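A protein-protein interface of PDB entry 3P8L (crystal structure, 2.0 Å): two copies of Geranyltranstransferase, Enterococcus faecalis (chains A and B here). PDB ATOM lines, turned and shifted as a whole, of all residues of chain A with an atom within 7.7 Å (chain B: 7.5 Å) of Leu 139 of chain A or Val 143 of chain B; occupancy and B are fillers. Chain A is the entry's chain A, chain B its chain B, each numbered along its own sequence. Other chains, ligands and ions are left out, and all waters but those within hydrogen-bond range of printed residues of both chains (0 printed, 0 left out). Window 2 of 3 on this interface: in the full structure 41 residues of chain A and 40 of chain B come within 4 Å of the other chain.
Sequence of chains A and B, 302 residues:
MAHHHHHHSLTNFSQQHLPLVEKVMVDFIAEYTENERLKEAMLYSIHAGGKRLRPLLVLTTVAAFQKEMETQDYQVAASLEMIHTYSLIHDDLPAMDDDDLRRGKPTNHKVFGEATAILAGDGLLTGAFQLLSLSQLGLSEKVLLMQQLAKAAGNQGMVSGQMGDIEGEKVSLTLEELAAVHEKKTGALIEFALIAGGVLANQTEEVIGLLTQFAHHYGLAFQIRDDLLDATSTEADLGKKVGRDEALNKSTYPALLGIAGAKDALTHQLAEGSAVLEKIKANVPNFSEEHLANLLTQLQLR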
ATOM      1  N   LEU A 132     -17.426  10.692 -27.844  1.00  0.00           N
ATOM      2  CA  LEU A 132     -18.869  10.865 -27.734  1.00  0.00           C
ATOM      3  C   LEU A 132     -19.439  12.006 -28.619  1.00  0.00           C
ATOM      4  O   LEU A 132     -20.481  11.829 -29.279  1.00  0.00           O
ATOM      5  CB  LEU A 132     -19.273  11.027 -26.265  1.00  0.00           C
ATOM      6  CG  LEU A 132     -20.733  10.814 -25.856  1.00  0.00           C
ATOM      7  CD1 LEU A 132     -21.276   9.463 -26.372  1.00  0.00           C
ATOM      8  CD2 LEU A 132     -20.863  10.869 -24.338  1.00  0.00           C
ATOM      9  N   SER A 133     -18.723  13.131 -28.671  1.00  0.00           N
ATOM     10  CA  SER A 133     -19.064  14.283 -29.532  1.00  0.00           C
ATOM     11  C   SER A 133     -18.989  13.977 -31.034  1.00  0.00           C
ATOM     12  O   SER A 133     -19.759  14.544 -31.839  1.00  0.00           O
ATOM     13  CB  SER A 133     -18.177  15.493 -29.190  1.00  0.00           C
ATOM     14  OG  SER A 133     -16.924  15.412 -29.830  1.00  0.00           O
ATOM     15  N   LEU A 134     -18.082  13.071 -31.398  1.00  0.00           N
ATOM     16  CA  LEU A 134     -17.904  12.638 -32.777  1.00  0.00           C
ATOM     17  C   LEU A 134     -18.624  11.318 -33.125  1.00  0.00           C
ATOM     18  O   LEU A 134     -18.445  10.796 -34.218  1.00  0.00           O
ATOM     19  CB  LEU A 134     -16.408  12.495 -33.082  1.00  0.00           C
ATOM     20  CG  LEU A 134     -15.605  13.797 -33.143  1.00  0.00           C
ATOM     21  CD1 LEU A 134     -14.129  13.499 -33.004  1.00  0.00           C
ATOM     22  CD2 LEU A 134     -15.895  14.589 -34.441  1.00  0.00           C
ATOM     23  N   SER A 135     -19.398  10.774 -32.188  1.00  0.00           N
ATOM     24  CA  SER A 135     -20.021   9.459 -32.369  1.00  0.00           C
ATOM     25  C   SER A 135     -21.204   9.457 -33.346  1.00  0.00           C
ATOM     26  O   SER A 135     -21.694  10.507 -33.752  1.00  0.00           O
ATOM     27  CB  SER A 135     -20.459   8.882 -31.019  1.00  0.00           C
ATOM     28  OG  SER A 135     -21.532   9.615 -30.464  1.00  0.00           O
ATOM     29  N   GLN A 136     -21.670   8.265 -33.699  1.00  0.00           N
ATOM     30  CA  GLN A 136     -22.774   8.097 -34.644  1.00  0.00           C
ATOM     31  C   GLN A 136     -24.162   8.424 -34.075  1.00  0.00           C
ATOM     32  O   GLN A 136     -25.164   8.165 -34.728  1.00  0.00           O
ATOM     33  CB  GLN A 136     -22.773   6.660 -35.166  1.00  0.00           C
ATOM     34  CG  GLN A 136     -22.845   6.551 -36.663  1.00  0.00           C
ATOM     35  CD  GLN A 136     -21.481   6.447 -37.276  1.00  0.00           C
ATOM     36  OE1 GLN A 136     -21.061   5.366 -37.689  1.00  0.00           O
ATOM     37  NE2 GLN A 136     -20.767   7.566 -37.335  1.00  0.00           N
ATOM     38  N   LEU A 137     -24.223   8.969 -32.859  1.00  0.00           N
ATOM     39  CA  LEU A 137     -25.489   9.362 -32.236  1.00  0.00           C
ATOM     40  C   LEU A 137     -26.097  10.571 -32.922  1.00  0.00           C
ATOM     41  O   LEU A 137     -25.368  11.450 -33.391  1.00  0.00           O
ATOM     42  CB  LEU A 137     -25.274   9.730 -30.767  1.00  0.00           C
ATOM     43  CG  LEU A 137     -24.895   8.632 -29.779  1.00  0.00           C
ATOM     44  CD1 LEU A 137     -24.662   9.237 -28.416  1.00  0.00           C
ATOM     45  CD2 LEU A 137     -26.002   7.591 -29.742  1.00  0.00           C
ATOM     46  N   GLY A 138     -27.428  10.626 -32.943  1.00  0.00           N
ATOM     47  CA  GLY A 138     -28.138  11.816 -33.403  1.00  0.00           C
ATOM     48  C   GLY A 138     -28.047  12.931 -32.376  1.00  0.00           C
ATOM     49  O   GLY A 138     -27.773  12.677 -31.202  1.00  0.00           O
ATOM     50  N   LEU A 139     -28.327  14.157 -32.813  1.00  0.00           N
ATOM     51  CA  LEU A 139     -28.005  15.370 -32.061  1.00  0.00           C
ATOM     52  C   LEU A 139     -28.525  15.440 -30.634  1.00  0.00           C
ATOM     53  O   LEU A 139     -27.770  15.804 -29.722  1.00  0.00           O
ATOM     54  CB  LEU A 139     -28.407  16.633 -32.842  1.00  0.00           C
ATOM     55  CG  LEU A 139     -27.616  16.997 -34.105  1.00  0.00           C
ATOM     56  CD1 LEU A 139     -28.360  18.083 -34.904  1.00  0.00           C
ATOM     57  CD2 LEU A 139     -26.208  17.480 -33.777  1.00  0.00           C
ATOM     58  N   SER A 140     -29.786  15.078 -30.423  1.00  0.00           N
ATOM     59  CA  SER A 140     -30.375  15.206 -29.086  1.00  0.00           C
ATOM     60  C   SER A 140     -29.931  14.106 -28.126  1.00  0.00           C
ATOM     61  O   SER A 140     -29.800  14.347 -26.919  1.00  0.00           O
ATOM     62  CB  SER A 140     -31.901  15.247 -29.159  1.00  0.00           C
ATOM     63  OG  SER A 140     -32.396  14.048 -29.718  1.00  0.00           O
ATOM     64  N   GLU A 141     -29.732  12.899 -28.662  1.00  0.00           N
ATOM     65  CA  GLU A 141     -29.238  11.767 -27.877  1.00  0.00           C
ATOM     66  C   GLU A 141     -27.795  12.029 -27.465  1.00  0.00           C
ATOM     67  O   GLU A 141     -27.393  11.718 -26.343  1.00  0.00           O
ATOM     68  CB  GLU A 141     -29.275  10.484 -28.704  1.00  0.00           C
ATOM     69  CG  GLU A 141     -30.616   9.812 -28.762  1.00  0.00           C
ATOM     70  CD  GLU A 141     -30.559   8.493 -29.516  1.00  0.00           C
ATOM     71  OE1 GLU A 141     -31.377   7.608 -29.189  1.00  0.00           O
ATOM     72  OE2 GLU A 141     -29.699   8.337 -30.422  1.00  0.00           O
ATOM     73  N   LYS A 142     -27.039  12.586 -28.407  1.00  0.00           N
ATOM     74  CA  LYS A 142     -25.651  12.960 -28.215  1.00  0.00           C
ATOM     75  C   LYS A 142     -25.539  13.914 -27.046  1.00  0.00           C
ATOM     76  O   LYS A 142     -24.780  13.651 -26.120  1.00  0.00           O
ATOM     77  CB  LYS A 142     -25.084  13.586 -29.487  1.00  0.00           C
ATOM     78  CG  LYS A 142     -23.581  13.810 -29.455  1.00  0.00           C
ATOM     79  CD  LYS A 142     -23.034  14.178 -30.825  1.00  0.00           C
ATOM     80  CE  LYS A 142     -22.842  12.942 -31.662  1.00  0.00           C
ATOM     81  NZ  LYS A 142     -22.029  13.245 -32.896  1.00  0.00           N
ATOM     82  N   VAL A 143     -26.349  14.973 -27.060  1.00  0.00           N
ATOM     83  CA  VAL A 143     -26.328  15.987 -26.013  1.00  0.00           C
ATOM     84  C   VAL A 143     -26.759  15.432 -24.664  1.00  0.00           C
ATOM     85  O   VAL A 143     -26.129  15.726 -23.650  1.00  0.00           O
ATOM     86  CB  VAL A 143     -27.149  17.257 -26.420  1.00  0.00           C
ATOM     87  CG1 VAL A 143     -27.494  18.155 -25.217  1.00  0.00           C
ATOM     88  CG2 VAL A 143     -26.394  18.053 -27.438  1.00  0.00           C
ATOM     89  N   LEU A 144     -27.800  14.595 -24.661  1.00  0.00           N
ATOM     90  CA  LEU A 144     -28.259  13.938 -23.441  1.00  0.00           C
ATOM     91  C   LEU A 144     -27.154  13.071 -22.821  1.00  0.00           C
ATOM     92  O   LEU A 144     -26.936  13.101 -21.618  1.00  0.00           O
ATOM     93  CB  LEU A 144     -29.509  13.076 -23.723  1.00  0.00           C
ATOM     94  CG  LEU A 144     -30.080  12.251 -22.563  1.00  0.00           C
ATOM     95  CD1 LEU A 144     -30.473  13.134 -21.381  1.00  0.00           C
ATOM     96  CD2 LEU A 144     -31.267  11.420 -23.039  1.00  0.00           C
ATOM     97  N   LEU A 145     -26.481  12.296 -23.651  1.00  0.00           N
ATOM     98  CA  LEU A 145     -25.489  11.353 -23.135  1.00  0.00           C
ATOM     99  C   LEU A 145     -24.209  12.079 -22.675  1.00  0.00           C
ATOM    100  O   LEU A 145     -23.555  11.622 -21.743  1.00  0.00           O
ATOM    101  CB  LEU A 145     -25.206  10.241 -24.153  1.00  0.00           C
ATOM    102  CG  LEU A 145     -26.338   9.205 -24.316  1.00  0.00           C
ATOM    103  CD1 LEU A 145     -25.859   8.011 -25.095  1.00  0.00           C
ATOM    104  CD2 LEU A 145     -26.899   8.740 -23.000  1.00  0.00           C
ATOM    105  N   MET A 146     -23.905  13.226 -23.288  1.00  0.00           N
ATOM    106  CA  MET A 146     -22.767  14.056 -22.871  1.00  0.00           C
ATOM    107  C   MET A 146     -23.079  14.699 -21.521  1.00  0.00           C
ATOM    108  O   MET A 146     -22.233  14.720 -20.623  1.00  0.00           O
ATOM    109  CB  MET A 146     -22.405  15.104 -23.941  1.00  0.00           C
ATOM    110  CG  MET A 146     -21.634  14.529 -25.152  1.00  0.00           C
ATOM    111  SD  MET A 146     -21.109  15.719 -26.425  1.00  0.00           S
ATOM    112  CE  MET A 146     -22.635  16.556 -26.819  1.00  0.00           C
ATOM    113  N   LEU B 132     -20.943  23.376 -20.943  1.00  0.00           N
ATOM    114  CA  LEU B 132     -21.219  23.458 -22.373  1.00  0.00           C
ATOM    115  C   LEU B 132     -22.411  22.585 -22.812  1.00  0.00           C
ATOM    116  O   LEU B 132     -23.195  22.983 -23.688  1.00  0.00           O
ATOM    117  CB  LEU B 132     -19.967  23.088 -23.170  1.00  0.00           C
ATOM    118  CG  LEU B 132     -19.795  23.638 -24.591  1.00  0.00           C
ATOM    119  CD1 LEU B 132     -20.154  25.124 -24.662  1.00  0.00           C
ATOM    120  CD2 LEU B 132     -18.363  23.400 -25.123  1.00  0.00           C
ATOM    121  N   LEU B 137     -27.110  26.991 -25.820  1.00  0.00           N
ATOM    122  CA  LEU B 137     -26.857  26.844 -27.242  1.00  0.00           C
ATOM    123  C   LEU B 137     -27.891  25.872 -27.796  1.00  0.00           C
ATOM    124  O   LEU B 137     -28.392  25.014 -27.063  1.00  0.00           O
ATOM    125  CB  LEU B 137     -25.463  26.264 -27.480  1.00  0.00           C
ATOM    126  CG  LEU B 137     -24.196  27.040 -27.126  1.00  0.00           C
ATOM    127  CD1 LEU B 137     -23.032  26.081 -26.946  1.00  0.00           C
ATOM    128  CD2 LEU B 137     -23.887  28.026 -28.216  1.00  0.00           C
ATOM    129  N   GLY B 138     -28.195  25.999 -29.086  1.00  0.00           N
ATOM    130  CA  GLY B 138     -29.028  25.020 -29.782  1.00  0.00           C
ATOM    131  C   GLY B 138     -28.208  23.768 -30.032  1.00  0.00           C
ATOM    132  O   GLY B 138     -26.986  23.824 -29.996  1.00  0.00           O
ATOM    133  N   LEU B 139     -28.880  22.651 -30.305  1.00  0.00           N
ATOM    134  CA  LEU B 139     -28.238  21.332 -30.413  1.00  0.00           C
ATOM    135  C   LEU B 139     -27.058  21.252 -31.386  1.00  0.00           C
ATOM    136  O   LEU B 139     -26.027  20.659 -31.062  1.00  0.00           O
ATOM    137  CB  LEU B 139     -29.266  20.250 -30.769  1.00  0.00           C
ATOM    138  CG  LEU B 139     -30.511  20.122 -29.893  1.00  0.00           C
ATOM    139  CD1 LEU B 139     -31.554  19.266 -30.597  1.00  0.00           C
ATOM    140  CD2 LEU B 139     -30.173  19.559 -28.512  1.00  0.00           C
ATOM    141  N   SER B 140     -27.201  21.853 -32.562  1.00  0.00           N
ATOM    142  CA  SER B 140     -26.185  21.733 -33.597  1.00  0.00           C
ATOM    143  C   SER B 140     -24.877  22.469 -33.257  1.00  0.00           C
ATOM    144  O   SER B 140     -23.778  21.974 -33.536  1.00  0.00           O
ATOM    145  CB  SER B 140     -26.729  22.206 -34.937  1.00  0.00           C
ATOM    146  OG  SER B 140     -25.898  21.742 -35.980  1.00  0.00           O
ATOM    147  N   GLU B 141     -25.015  23.642 -32.645  1.00  0.00           N
ATOM    148  CA  GLU B 141     -23.878  24.455 -32.246  1.00  0.00           C
ATOM    149  C   GLU B 141     -23.277  23.934 -30.948  1.00  0.00           C
ATOM    150  O   GLU B 141     -22.094  24.104 -30.716  1.00  0.00           O
ATOM    151  CB  GLU B 141     -24.298  25.913 -32.051  1.00  0.00           C
ATOM    152  CG  GLU B 141     -24.660  26.642 -33.340  1.00  0.00           C
ATOM    153  CD  GLU B 141     -25.708  27.729 -33.129  1.00  0.00           C
ATOM    154  OE1 GLU B 141     -26.153  28.315 -34.140  1.00  0.00           O
ATOM    155  OE2 GLU B 141     -26.090  27.992 -31.962  1.00  0.00           O
ATOM    156  N   LYS B 142     -24.108  23.333 -30.098  1.00  0.00           N
ATOM    157  CA  LYS B 142     -23.664  22.758 -28.834  1.00  0.00           C
ATOM    158  C   LYS B 142     -22.732  21.584 -29.116  1.00  0.00           C
ATOM    159  O   LYS B 142     -21.667  21.478 -28.508  1.00  0.00           O
ATOM    160  CB  LYS B 142     -24.864  22.296 -28.029  1.00  0.00           C
ATOM    161  CG  LYS B 142     -24.551  21.691 -26.684  1.00  0.00           C
ATOM    162  CD  LYS B 142     -25.816  21.486 -25.890  1.00  0.00           C
ATOM    163  CE  LYS B 142     -26.341  22.781 -25.346  1.00  0.00           C
ATOM    164  NZ  LYS B 142     -27.326  22.503 -24.289  1.00  0.00           N
ATOM    165  N   VAL B 143     -23.132  20.746 -30.074  1.00  0.00           N
ATOM    166  CA  VAL B 143     -22.356  19.599 -30.522  1.00  0.00           C
ATOM    167  C   VAL B 143     -21.075  20.034 -31.227  1.00  0.00           C
ATOM    168  O   VAL B 143     -20.000  19.500 -30.937  1.00  0.00           O
ATOM    169  CB  VAL B 143     -23.213  18.663 -31.403  1.00  0.00           C
ATOM    170  CG1 VAL B 143     -22.361  17.706 -32.231  1.00  0.00           C
ATOM    171  CG2 VAL B 143     -24.186  17.898 -30.524  1.00  0.00           C
ATOM    172  N   LEU B 144     -21.179  21.028 -32.109  1.00  0.00           N
ATOM    173  CA  LEU B 144     -20.006  21.569 -32.794  1.00  0.00           C
ATOM    174  C   LEU B 144     -18.953  22.113 -31.812  1.00  0.00           C
ATOM    175  O   LEU B 144     -17.766  21.824 -31.949  1.00  0.00           O
ATOM    176  CB  LEU B 144     -20.406  22.654 -33.805  1.00  0.00           C
ATOM    177  CG  LEU B 144     -19.271  23.321 -34.608  1.00  0.00           C
ATOM    178  CD1 LEU B 144     -18.479  22.318 -35.455  1.00  0.00           C
ATOM    179  CD2 LEU B 144     -19.796  24.460 -35.491  1.00  0.00           C
ATOM    180  N   LEU B 145     -19.388  22.885 -30.826  1.00  0.00           N
ATOM    181  CA  LEU B 145     -18.436  23.513 -29.907  1.00  0.00           C
ATOM    182  C   LEU B 145     -17.835  22.523 -28.900  1.00  0.00           C
ATOM    183  O   LEU B 145     -16.669  22.666 -28.519  1.00  0.00           O
ATOM    184  CB  LEU B 145     -19.074  24.706 -29.201  1.00  0.00           C
ATOM    185  CG  LEU B 145     -19.408  25.935 -30.066  1.00  0.00           C
ATOM    186  CD1 LEU B 145     -19.843  27.060 -29.167  1.00  0.00           C
ATOM    187  CD2 LEU B 145     -18.228  26.363 -30.942  1.00  0.00           C
ATOM    188  N   MET B 146     -18.630  21.540 -28.459  1.00  0.00           N
ATOM    189  CA  MET B 146     -18.108  20.452 -27.625  1.00  0.00           C
ATOM    190  C   MET B 146     -17.004  19.706 -28.383  1.00  0.00           C
ATOM    191  O   MET B 146     -15.911  19.476 -27.842  1.00  0.00           O
ATOM    192  CB  MET B 146     -19.224  19.519 -27.137  1.00  0.00           C
ATOM    193  CG  MET B 146     -20.060  20.129 -26.005  1.00  0.00           C
ATOM    194  SD  MET B 146     -21.227  19.033 -25.191  1.00  0.00           S
ATOM    195  CE  MET B 146     -20.099  18.097 -24.153  1.00  0.00           C
ATOM    196  N   GLN B 147     -17.257  19.384 -29.654  1.00  0.00           N
ATOM    197  CA  GLN B 147     -16.237  18.762 -30.513  1.00  0.00           C
ATOM    198  C   GLN B 147     -14.988  19.659 -30.585  1.00  0.00           C
ATOM    199  O   GLN B 147     -13.844  19.186 -30.440  1.00  0.00           O
ATOM    200  CB  GLN B 147     -16.749  18.563 -31.953  1.00  0.00           C
ATOM    201  CG  GLN B 147     -17.859  17.525 -32.137  1.00  0.00           C
ATOM    202  CD  GLN B 147     -18.499  17.579 -33.532  1.00  0.00           C
ATOM    203  OE1 GLN B 147     -18.333  18.548 -34.270  1.00  0.00           O
ATOM    204  NE2 GLN B 147     -19.220  16.530 -33.889  1.00  0.00           N
ATOM    205  N   GLN B 148     -15.207  20.952 -30.815  1.00  0.00           N
ATOM    206  CA  GLN B 148     -14.089  21.885 -30.971  1.00  0.00           C
ATOM    207  C   GLN B 148     -13.317  22.081 -29.676  1.00  0.00           C
ATOM    208  O   GLN B 148     -12.091  22.205 -29.701  1.00  0.00           O
ATOM    209  CB  GLN B 148     -14.559  23.230 -31.547  1.00  0.00           C
ATOM    210  CG  GLN B 148     -14.995  23.138 -33.017  1.00  0.00           C
ATOM    211  CD  GLN B 148     -13.874  22.722 -33.933  1.00  0.00           C
ATOM    212  OE1 GLN B 148     -12.790  23.302 -33.906  1.00  0.00           O
ATOM    213  NE2 GLN B 148     -14.122  21.708 -34.750  1.00  0.00           N
ATOM    214  N   LEU B 149     -14.029  22.119 -28.561  1.00  0.00           N
ATOM    215  CA  LEU B 149     -13.389  22.286 -27.263  1.00  0.00           C
ATOM    216  C   LEU B 149     -12.579  21.034 -26.933  1.00  0.00           C
ATOM    217  O   LEU B 149     -11.457  21.147 -26.451  1.00  0.00           O
ATOM    218  CB  LEU B 149     -14.398  22.591 -26.146  1.00  0.00           C
ATOM    219  CG  LEU B 149     -13.766  22.963 -24.799  1.00  0.00           C
ATOM    220  CD1 LEU B 149     -12.855  24.225 -24.926  1.00  0.00           C
ATOM    221  CD2 LEU B 149     -14.812  23.143 -23.711  1.00  0.00           C
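O of Ser 133 of chain A lies within hydrogen-bond range of NE2 of Gln 147 of chain B (2.9 Å).
The side-chain sulfur of Met 146 of chain A sits close to the side-chain sulfur of Met 146 of chain B.
O of Ser 133 of chain A lies within hydrogen-bond range of NZ of Lys 142 of chain A (2.8 Å).
O of Ser 135 of chain A is in hydrogen-bond range of NZ of Lys 142 of chain A (2.9 Å).
Of the 15 printed residues of chain A, 6 touch a printed residue of chain B.
Hydrophobic or aromatic side chains of chain A within 4 Å of the printed part of chain B: Leu 134, Leu 139, Val 143 and Met 146.
Of the 14 printed residues of chain B, 4 touch a printed residue of chain A.
Printed residues of chain B that touch a printed residue of chain A: Lys 142, Val 143, Met 146 and Gln 147.
Hydrophobic or aromatic side chains of chain B within 4 Å of the printed part of chain A: Val 143 and Met 146.
Among the printed residues, 7 pairs touch across the chains.
Leu 134 of chain A touches Gln 147 of chain B.
Val 143 of chain B touches Leu 139 of chain A.
Lys 142 of chain A touches Val 143 of chain B (CD to CG1, 3.9 Å).
Val 143 of chain A touches Lys 142 of chain B.
CG2 of Val 143 of chain A touches CG2 of Val 143 of chain B, at 3.8 Å.
Leu 139 of chain A touches just one residue of chain B: Val 143.
Val 143 of chain B touches just these residues of chain A: Leu 139, Lys 142 and Val 143.
Of the printed residues of chain A, Gln 147 of chain B touches Ser 133 and Leu 134.
Of the printed residues of chain B, Ser 133 of chain A touches Gln 147.
Of the printed residues of chain B, Lys 142 of chain A touches Val 143.
The nearest residue of chain B that does not touch Leu 139 of chain A is Leu 139 of chain B (4.2 Å).
Leu 139 of chain A touches Val 143 of chain B, but with the chains exchanged Val 143 of chain A does not touch Leu 139 of chain B (4.2 Å).
Lys 142 of chain A touches Val 143 of chain B, and with the chains exchanged Val 143 of chain A touches Lys 142 of chain B.
Val 143 of chain B touches its own counterpart, Val 143 of chain A.
Met 146 of chain B touches its own counterpart, Met 146 of chain A.
11 positions are printed for both chains.
Of the 7 pairs that touch across the chains among the printed residues, 4 have their exchanged pair printed and touching as well.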
